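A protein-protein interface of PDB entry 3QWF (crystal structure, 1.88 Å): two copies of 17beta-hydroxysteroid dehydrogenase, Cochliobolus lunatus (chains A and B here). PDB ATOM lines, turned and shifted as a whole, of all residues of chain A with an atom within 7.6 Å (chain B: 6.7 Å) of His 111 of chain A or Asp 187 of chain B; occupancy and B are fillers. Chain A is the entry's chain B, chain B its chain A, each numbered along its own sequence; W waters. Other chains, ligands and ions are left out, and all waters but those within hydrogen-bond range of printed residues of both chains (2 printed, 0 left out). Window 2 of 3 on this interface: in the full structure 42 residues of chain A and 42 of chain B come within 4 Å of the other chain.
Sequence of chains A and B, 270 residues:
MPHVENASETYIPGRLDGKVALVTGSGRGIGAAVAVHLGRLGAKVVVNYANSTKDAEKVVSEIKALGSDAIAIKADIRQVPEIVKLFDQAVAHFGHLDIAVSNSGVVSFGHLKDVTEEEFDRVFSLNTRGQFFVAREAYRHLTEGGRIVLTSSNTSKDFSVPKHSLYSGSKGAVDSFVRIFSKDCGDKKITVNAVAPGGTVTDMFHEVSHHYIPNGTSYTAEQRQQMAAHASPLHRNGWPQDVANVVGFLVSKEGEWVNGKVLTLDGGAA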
ATOM      1  N   PHE A 109      22.878 -14.267   9.513  1.00  0.00           N
ATOM      2  CA  PHE A 109      21.436 -14.162   9.669  1.00  0.00           C
ATOM      3  C   PHE A 109      20.740 -14.527   8.370  1.00  0.00           C
ATOM      4  O   PHE A 109      21.211 -14.197   7.282  1.00  0.00           O
ATOM      5  CB  PHE A 109      21.017 -12.742  10.100  1.00  0.00           C
ATOM      6  CG  PHE A 109      21.198 -12.488  11.575  1.00  0.00           C
ATOM      7  CD1 PHE A 109      22.434 -12.085  12.080  1.00  0.00           C
ATOM      8  CD2 PHE A 109      20.131 -12.657  12.456  1.00  0.00           C
ATOM      9  CE1 PHE A 109      22.609 -11.857  13.465  1.00  0.00           C
ATOM     10  CE2 PHE A 109      20.288 -12.433  13.835  1.00  0.00           C
ATOM     11  CZ  PHE A 109      21.532 -12.028  14.341  1.00  0.00           C
ATOM     12  N   GLY A 110      19.618 -15.220   8.506  1.00  0.00           N
ATOM     13  CA  GLY A 110      18.768 -15.580   7.378  1.00  0.00           C
ATOM     14  C   GLY A 110      17.650 -16.478   7.864  1.00  0.00           C
ATOM     15  O   GLY A 110      17.851 -17.302   8.756  1.00  0.00           O
ATOM     16  N   HIS A 111      16.463 -16.290   7.307  1.00  0.00           N
ATOM     17  CA  HIS A 111      15.367 -17.218   7.518  1.00  0.00           C
ATOM     18  C   HIS A 111      15.809 -18.596   7.012  1.00  0.00           C
ATOM     19  O   HIS A 111      16.426 -18.712   5.938  1.00  0.00           O
ATOM     20  CB  HIS A 111      14.134 -16.731   6.757  1.00  0.00           C
ATOM     21  CG  HIS A 111      12.850 -17.393   7.162  1.00  0.00           C
ATOM     22  ND1 HIS A 111      12.585 -18.724   6.918  1.00  0.00           N
ATOM     23  CD2 HIS A 111      11.740 -16.892   7.756  1.00  0.00           C
ATOM     24  CE1 HIS A 111      11.367 -19.013   7.338  1.00  0.00           C
ATOM     25  NE2 HIS A 111      10.835 -17.920   7.856  1.00  0.00           N
ATOM     26  N   LEU A 112      15.488 -19.626   7.792  1.00  0.00           N
ATOM     27  CA  LEU A 112      15.754 -21.025   7.426  1.00  0.00           C
ATOM     28  C   LEU A 112      15.516 -21.329   5.940  1.00  0.00           C
ATOM     29  O   LEU A 112      16.325 -21.997   5.290  1.00  0.00           O
ATOM     30  CB  LEU A 112      14.911 -21.964   8.305  1.00  0.00           C
ATOM     31  CG  LEU A 112      14.772 -23.443   7.886  1.00  0.00           C
ATOM     32  CD1 LEU A 112      16.106 -24.192   7.869  1.00  0.00           C
ATOM     33  CD2 LEU A 112      13.725 -24.190   8.728  1.00  0.00           C
ATOM     34  N   LYS A 113      14.411 -20.807   5.413  1.00  0.00           N
ATOM     35  CA  LYS A 113      13.984 -21.053   4.039  1.00  0.00           C
ATOM     36  C   LYS A 113      14.951 -20.558   2.952  1.00  0.00           C
ATOM     37  O   LYS A 113      14.837 -20.974   1.799  1.00  0.00           O
ATOM     38  CB  LYS A 113      12.601 -20.434   3.812  1.00  0.00           C
ATOM     39  CG  LYS A 113      12.604 -18.919   3.697  1.00  0.00           C
ATOM     40  CD  LYS A 113      11.210 -18.340   3.495  1.00  0.00           C
ATOM     41  CE  LYS A 113      11.275 -16.822   3.469  1.00  0.00           C
ATOM     42  NZ  LYS A 113      11.835 -16.321   2.170  1.00  0.00           N
ATOM     43  N   ASP A 114      15.872 -19.673   3.331  1.00  0.00           N
ATOM     44  CA  ASP A 114      16.801 -19.021   2.405  1.00  0.00           C
ATOM     45  C   ASP A 114      18.260 -19.413   2.613  1.00  0.00           C
ATOM     46  O   ASP A 114      19.129 -18.977   1.855  1.00  0.00           O
ATOM     47  CB  ASP A 114      16.691 -17.492   2.520  1.00  0.00           C
ATOM     48  CG  ASP A 114      15.322 -16.973   2.167  1.00  0.00           C
ATOM     49  OD1 ASP A 114      14.712 -17.483   1.208  1.00  0.00           O
ATOM     50  OD2 ASP A 114      14.857 -16.041   2.857  1.00  0.00           O
ATOM     51  N   VAL A 115      18.537 -20.213   3.641  1.00  0.00           N
ATOM     52  CA  VAL A 115      19.915 -20.596   3.937  1.00  0.00           C
ATOM     53  C   VAL A 115      20.433 -21.578   2.875  1.00  0.00           C
ATOM     54  O   VAL A 115      19.796 -22.595   2.571  1.00  0.00           O
ATOM     55  CB  VAL A 115      20.097 -21.136   5.377  1.00  0.00           C
ATOM     56  CG1 VAL A 115      21.545 -21.554   5.630  1.00  0.00           C
ATOM     57  CG2 VAL A 115      19.664 -20.078   6.401  1.00  0.00           C
ATOM     58  N   THR A 116      21.573 -21.220   2.291  1.00  0.00           N
ATOM     59  CA  THR A 116      22.192 -21.990   1.225  1.00  0.00           C
ATOM     60  C   THR A 116      23.208 -22.972   1.806  1.00  0.00           C
ATOM     61  O   THR A 116      23.659 -22.818   2.939  1.00  0.00           O
ATOM     62  CB  THR A 116      22.946 -21.065   0.249  1.00  0.00           C
ATOM     63  OG1 THR A 116      23.968 -20.363   0.967  1.00  0.00           O
ATOM     64  CG2 THR A 116      22.001 -20.059  -0.424  1.00  0.00           C
ATOM     65  N   PRO A 162      14.972 -14.544  15.931  1.00  0.00           N
ATOM     66  CA  PRO A 162      14.502 -15.027  14.629  1.00  0.00           C
ATOM     67  C   PRO A 162      15.618 -14.942  13.580  1.00  0.00           C
ATOM     68  O   PRO A 162      16.510 -14.087  13.692  1.00  0.00           O
ATOM     69  CB  PRO A 162      13.378 -14.053  14.278  1.00  0.00           C
ATOM     70  CG  PRO A 162      12.864 -13.572  15.606  1.00  0.00           C
ATOM     71  CD  PRO A 162      14.066 -13.533  16.512  1.00  0.00           C
ATOM     72  N   LYS A 163      15.577 -15.840  12.595  1.00  0.00           N
ATOM     73  CA  LYS A 163      16.501 -15.814  11.455  1.00  0.00           C
ATOM     74  C   LYS A 163      17.967 -15.980  11.867  1.00  0.00           C
ATOM     75  O   LYS A 163      18.867 -15.533  11.167  1.00  0.00           O
ATOM     76  CB  LYS A 163      16.309 -14.531  10.617  1.00  0.00           C
ATOM     77  CG  LYS A 163      14.908 -14.341  10.045  1.00  0.00           C
ATOM     78  CD  LYS A 163      14.809 -13.011   9.308  1.00  0.00           C
ATOM     79  CE  LYS A 163      13.458 -12.813   8.659  1.00  0.00           C
ATOM     80  NZ  LYS A 163      12.359 -12.716   9.657  1.00  0.00           N
ATOM     81  N   HIS A 164      18.205 -16.666  12.985  1.00  0.00           N
ATOM     82  CA  HIS A 164      19.547 -16.802  13.532  1.00  0.00           C
ATOM     83  C   HIS A 164      19.884 -18.269  13.802  1.00  0.00           C
ATOM     84  O   HIS A 164      20.735 -18.568  14.634  1.00  0.00           O
ATOM     85  CB  HIS A 164      19.647 -15.984  14.824  1.00  0.00           C
ATOM     86  CG  HIS A 164      21.037 -15.554  15.182  1.00  0.00           C
ATOM     87  ND1 HIS A 164      21.979 -15.195  14.241  1.00  0.00           N
ATOM     88  CD2 HIS A 164      21.624 -15.370  16.388  1.00  0.00           C
ATOM     89  CE1 HIS A 164      23.094 -14.834  14.851  1.00  0.00           C
ATOM     90  NE2 HIS A 164      22.905 -14.928  16.153  1.00  0.00           N
ATOM     91  N   SER A 165      19.212 -19.182  13.101  1.00  0.00           N
ATOM     92  CA  SER A 165      19.332 -20.616  13.430  1.00  0.00           C
ATOM     93  C   SER A 165      20.706 -21.195  13.139  1.00  0.00           C
ATOM     94  O   SER A 165      21.253 -21.960  13.948  1.00  0.00           O
ATOM     95  CB  SER A 165      18.244 -21.443  12.729  1.00  0.00           C
ATOM     96  OG  SER A 165      18.385 -21.385  11.320  1.00  0.00           O
ATOM     97  N   PHE B 132      19.631 -30.108   9.114  1.00  0.00           N
ATOM     98  CA  PHE B 132      19.334 -28.697   8.889  1.00  0.00           C
ATOM     99  C   PHE B 132      18.602 -28.516   7.552  1.00  0.00           C
ATOM    100  O   PHE B 132      17.599 -27.795   7.468  1.00  0.00           O
ATOM    101  CB  PHE B 132      20.623 -27.864   8.917  1.00  0.00           C
ATOM    102  CG  PHE B 132      20.396 -26.400   8.646  1.00  0.00           C
ATOM    103  CD1 PHE B 132      20.317 -25.927   7.338  1.00  0.00           C
ATOM    104  CD2 PHE B 132      20.268 -25.500   9.705  1.00  0.00           C
ATOM    105  CE1 PHE B 132      20.079 -24.571   7.091  1.00  0.00           C
ATOM    106  CE2 PHE B 132      20.034 -24.145   9.471  1.00  0.00           C
ATOM    107  CZ  PHE B 132      19.939 -23.681   8.168  1.00  0.00           C
ATOM    108  N   ARG B 136      14.938 -27.252   6.239  1.00  0.00           N
ATOM    109  CA  ARG B 136      14.720 -26.242   5.169  1.00  0.00           C
ATOM    110  C   ARG B 136      13.730 -26.712   4.106  1.00  0.00           C
ATOM    111  O   ARG B 136      12.812 -25.969   3.738  1.00  0.00           O
ATOM    112  CB  ARG B 136      16.042 -25.847   4.504  1.00  0.00           C
ATOM    113  CG  ARG B 136      15.935 -24.670   3.526  1.00  0.00           C
ATOM    114  CD  ARG B 136      17.198 -24.526   2.686  1.00  0.00           C
ATOM    115  NE  ARG B 136      17.192 -25.458   1.564  1.00  0.00           N
ATOM    116  CZ  ARG B 136      18.100 -25.487   0.589  1.00  0.00           C
ATOM    117  NH1 ARG B 136      19.117 -24.630   0.581  1.00  0.00           N
ATOM    118  NH2 ARG B 136      17.989 -26.381  -0.385  1.00  0.00           N
ATOM    119  N   TYR B 139      10.134 -27.033   5.616  1.00  0.00           N
ATOM    120  CA  TYR B 139       9.495 -25.708   5.573  1.00  0.00           C
ATOM    121  C   TYR B 139       9.036 -25.366   4.163  1.00  0.00           C
ATOM    122  O   TYR B 139       7.881 -24.968   3.947  1.00  0.00           O
ATOM    123  CB  TYR B 139      10.419 -24.605   6.111  1.00  0.00           C
ATOM    124  CG  TYR B 139       9.776 -23.235   6.046  1.00  0.00           C
ATOM    125  CD1 TYR B 139       8.999 -22.762   7.099  1.00  0.00           C
ATOM    126  CD2 TYR B 139       9.917 -22.426   4.915  1.00  0.00           C
ATOM    127  CE1 TYR B 139       8.392 -21.516   7.035  1.00  0.00           C
ATOM    128  CE2 TYR B 139       9.311 -21.173   4.848  1.00  0.00           C
ATOM    129  CZ  TYR B 139       8.553 -20.731   5.911  1.00  0.00           C
ATOM    130  OH  TYR B 139       7.953 -19.496   5.859  1.00  0.00           O
ATOM    131  N   GLU B 144       0.491 -25.429   5.730  1.00  0.00           N
ATOM    132  CA  GLU B 144       0.307 -24.620   6.935  1.00  0.00           C
ATOM    133  C   GLU B 144      -0.202 -25.489   8.079  1.00  0.00           C
ATOM    134  O   GLU B 144      -1.048 -26.360   7.864  1.00  0.00           O
ATOM    135  CB  GLU B 144      -0.696 -23.494   6.653  1.00  0.00           C
ATOM    136  CG  GLU B 144      -0.162 -22.407   5.720  1.00  0.00           C
ATOM    137  CD  GLU B 144       0.299 -21.147   6.460  1.00  0.00           C
ATOM    138  OE1 GLU B 144      -0.091 -20.952   7.639  1.00  0.00           O
ATOM    139  OE2 GLU B 144       1.033 -20.337   5.844  1.00  0.00           O
ATOM    140  N   SER B 182      11.703 -22.929  15.275  1.00  0.00           N
ATOM    141  CA  SER B 182      10.314 -22.716  15.703  1.00  0.00           C
ATOM    142  C   SER B 182       9.872 -21.275  15.475  1.00  0.00           C
ATOM    143  O   SER B 182       8.694 -21.032  15.224  1.00  0.00           O
ATOM    144  CB  SER B 182      10.075 -23.129  17.161  1.00  0.00           C
ATOM    145  OG  SER B 182      10.832 -22.359  18.081  1.00  0.00           O
ATOM    146  N   LYS B 183      10.820 -20.336  15.552  1.00  0.00           N
ATOM    147  CA  LYS B 183      10.530 -18.927  15.330  1.00  0.00           C
ATOM    148  C   LYS B 183      10.258 -18.673  13.844  1.00  0.00           C
ATOM    149  O   LYS B 183       9.183 -18.170  13.485  1.00  0.00           O
ATOM    150  CB  LYS B 183      11.675 -18.039  15.845  1.00  0.00           C
ATOM    151  CG  LYS B 183      12.153 -18.390  17.272  1.00  0.00           C
ATOM    152  CD  LYS B 183      11.077 -18.113  18.338  1.00  0.00           C
ATOM    153  CE  LYS B 183      11.593 -18.457  19.737  1.00  0.00           C
ATOM    154  NZ  LYS B 183      11.683 -19.959  19.917  1.00  0.00           N
ATOM    155  N   ASP B 184      11.220 -19.054  12.998  1.00  0.00           N
ATOM    156  CA  ASP B 184      11.103 -18.948  11.543  1.00  0.00           C
ATOM    157  C   ASP B 184       9.865 -19.650  10.975  1.00  0.00           C
ATOM    158  O   ASP B 184       9.105 -19.061  10.199  1.00  0.00           O
ATOM    159  CB  ASP B 184      12.365 -19.505  10.879  1.00  0.00           C
ATOM    160  CG  ASP B 184      13.587 -18.607  11.080  1.00  0.00           C
ATOM    161  OD1 ASP B 184      13.503 -17.578  11.787  1.00  0.00           O
ATOM    162  OD2 ASP B 184      14.640 -18.933  10.506  1.00  0.00           O
ATOM    163  N   CYS B 185       9.660 -20.900  11.375  1.00  0.00           N
ATOM    164  CA  CYS B 185       8.576 -21.719  10.832  1.00  0.00           C
ATOM    165  C   CYS B 185       7.194 -21.344  11.343  1.00  0.00           C
ATOM    166  O   CYS B 185       6.196 -21.834  10.821  1.00  0.00           O
ATOM    167  CB  CYS B 185       8.844 -23.190  11.153  1.00  0.00           C
ATOM    168  SG  CYS B 185      10.286 -23.852  10.327  1.00  0.00           S
ATOM    169  N   GLY B 186       7.133 -20.491  12.366  1.00  0.00           N
ATOM    170  CA  GLY B 186       5.858 -19.994  12.892  1.00  0.00           C
ATOM    171  C   GLY B 186       5.063 -19.209  11.855  1.00  0.00           C
ATOM    172  O   GLY B 186       3.837 -19.066  11.964  1.00  0.00           O
ATOM    173  N   ASP B 187       5.745 -18.704  10.834  1.00  0.00           N
ATOM    174  CA  ASP B 187       5.022 -17.940   9.816  1.00  0.00           C
ATOM    175  C   ASP B 187       4.200 -18.823   8.849  1.00  0.00           C
ATOM    176  O   ASP B 187       3.405 -18.315   8.059  1.00  0.00           O
ATOM    177  CB  ASP B 187       5.914 -16.887   9.124  1.00  0.00           C
ATOM    178  CG  ASP B 187       7.034 -17.487   8.317  1.00  0.00           C
ATOM    179  OD1 ASP B 187       6.822 -18.567   7.728  1.00  0.00           O
ATOM    180  OD2 ASP B 187       8.127 -16.858   8.257  1.00  0.00           O
ATOM    181  N   LYS B 188       4.382 -20.140   8.955  1.00  0.00           N
ATOM    182  CA  LYS B 188       3.476 -21.125   8.354  1.00  0.00           C
ATOM    183  C   LYS B 188       2.720 -21.954   9.413  1.00  0.00           C
ATOM    184  O   LYS B 188       2.110 -22.971   9.079  1.00  0.00           O
ATOM    185  CB  LYS B 188       4.250 -22.049   7.400  1.00  0.00           C
ATOM    186  CG  LYS B 188       4.528 -21.442   6.011  1.00  0.00           C
ATOM    187  CD  LYS B 188       5.463 -22.314   5.163  1.00  0.00           C
ATOM    188  CE  LYS B 188       4.720 -23.456   4.475  1.00  0.00           C
ATOM    189  NZ  LYS B 188       5.314 -23.865   3.144  1.00  0.00           N
ATOM    190  N   LYS B 189       2.757 -21.512  10.677  1.00  0.00           N
ATOM    191  CA  LYS B 189       2.226 -22.270  11.835  1.00  0.00           C
ATOM    192  C   LYS B 189       2.768 -23.709  11.949  1.00  0.00           C
ATOM    193  O   LYS B 189       2.062 -24.632  12.382  1.00  0.00           O
ATOM    194  CB  LYS B 189       0.694 -22.274  11.903  1.00  0.00           C
ATOM    195  CG  LYS B 189       0.012 -20.904  11.742  1.00  0.00           C
ATOM    196  CD  LYS B 189       0.299 -19.982  12.922  1.00  0.00           C
ATOM    197  CE  LYS B 189      -0.425 -18.636  12.764  1.00  0.00           C
ATOM    198  NZ  LYS B 189      -1.890 -18.820  12.672  1.00  0.00           N
ATOM    199  N   ILE B 190       4.013 -23.890  11.535  1.00  0.00           N
ATOM    200  CA  ILE B 190       4.663 -25.179  11.629  1.00  0.00           C
ATOM    201  C   ILE B 190       5.472 -25.255  12.928  1.00  0.00           C
ATOM    202  O   ILE B 190       6.353 -24.432  13.170  1.00  0.00           O
ATOM    203  CB  ILE B 190       5.588 -25.432  10.422  1.00  0.00           C
ATOM    204  CG1 ILE B 190       4.769 -25.504   9.118  1.00  0.00           C
ATOM    205  CG2 ILE B 190       6.383 -26.737  10.621  1.00  0.00           C
ATOM    206  CD1 ILE B 190       5.632 -25.376   7.864  1.00  0.00           C
HETATM  207  O   HOH W   1      17.183 -19.092  10.805  1.00  0.00           O
HETATM  208  O   HOH W   2      11.749 -15.248  11.064  1.00  0.00           O
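His 111 of chain A touches three residues of chain B.
Printed residues of chain B within 4 Å of Lys 113 of chain A: Tyr 139 (3.5 Å).
Printed residues of chain B within 4 Å of Pro 162 of chain A: Asp 184.
Printed residues of chain A within 4 Å of Arg 136 of chain B: Leu 112 (3.2 Å) and Val 115 (2.9 Å).
Printed residues of chain A within 4 Å of Tyr 139 of chain B: His 111 (3.6 Å) and Lys 113 (3.5 Å).
Of the printed residues of chain A, Asp 184 of chain B touches His 111 (3.1 Å), Leu 112 (2.9 Å), Pro 162 (3.8 Å) and Lys 163 (2.8 Å).
No residue of chain A comes within 4 Å of Gly 186 of chain B.
Asp 187 of chain B touches one residue of chain A.
The nearest residue of chain B that does not touch His 111 of chain A is Cys 185 of chain B (4.8 Å).
The nearest residue of chain A that does not touch Asp 187 of chain B is Lys 113 of chain A (5.7 Å).
Of the 13 printed residues of chain B, 6 touch a printed residue of chain A.
Hydrophobic or aromatic side chains of chain B that line the printed part of chain A: Phe 132 and Tyr 139.
Among the printed residues, no Asp or Glu carboxylate lies within 4 Å of a Lys or Arg side-chain nitrogen of the other chain.
CZ of Tyr 139 of chain B touches CE1 of His 111 of chain A, at 3.6 Å.
Phe 132 of chain B touches Leu 112 of chain A.
Leu 112 of chain A touches Arg 136 of chain B.
CD2 of Leu 112 of chain A touches SG of Cys 185 of chain B, at 3.8 Å.
CD2 of Tyr 139 of chain B touches CB of Lys 113 of chain A, at 3.5 Å.
CE1 of Phe 132 of chain B touches CG1 of Val 115 of chain A, 3.7 Å away.
Asp 184 of chain B touches Pro 162 of chain A.
OG of Ser 165 of chain A touches CE2 of Phe 132 of chain B, at 3.7 Å.
Water W1 lies within hydrogen-bond range of OD2 of Asp 184 of chain B (2.6 Å), OG of Ser 165 of chain A (2.6 Å), O of Gly 110 of chain A (2.8 Å), N of His 164 of chain A (3.4 Å) and N of Leu 112 of chain A (3.5 Å).
Water W2 lies within hydrogen-bond range of the side-chain amino group (NZ) of Lys 163 of chain A and the side-chain carboxylate (OD1) of Asp 184 of chain B.
No position is printed for both chains.
The backbone carbonyl oxygen of Tyr 139 of chain B is in hydrogen-bond range of the side-chain amino group of Lys 188 of chain B (2.9 Å).
The backbone carbonyl oxygen (O) of Cys 185 of chain B is in hydrogen-bond range of the backbone NH (N) of Ile 190 of chain B.
The backbone carbonyl oxygen (O) of Lys 163 of chain A sits at hydrogen-bond distance from the backbone NH (N) of Gly 110 of chain A.
ND1 of His 111 of chain A sits close to N of Lys 113 of chain A (3.2 Å).
NZ of Lys 113 of chain A is in salt-bridge range of OD2 of Asp 114 of chain A (3.1 Å).
NH1 of Arg 136 of chain B sits at hydrogen-bond distance from O of Val 115 of chain A (2.9 Å).
O of Asp 184 of chain B is in hydrogen-bond range of NE2 of His 111 of chain A (3.1 Å).
N of Leu 112 of chain A is in hydrogen-bond range of OD2 of Asp 184 of chain B, at 2.9 Å.
OD1 of Asp 184 of chain B is in hydrogen-bond range of N of Lys 163 of chain A, 2.8 Å away.
A ring nitrogen (NE2) of His 111 of chain A lies within hydrogen-bond range of the side-chain carboxylate (OD2) of Asp 187 of chain B.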
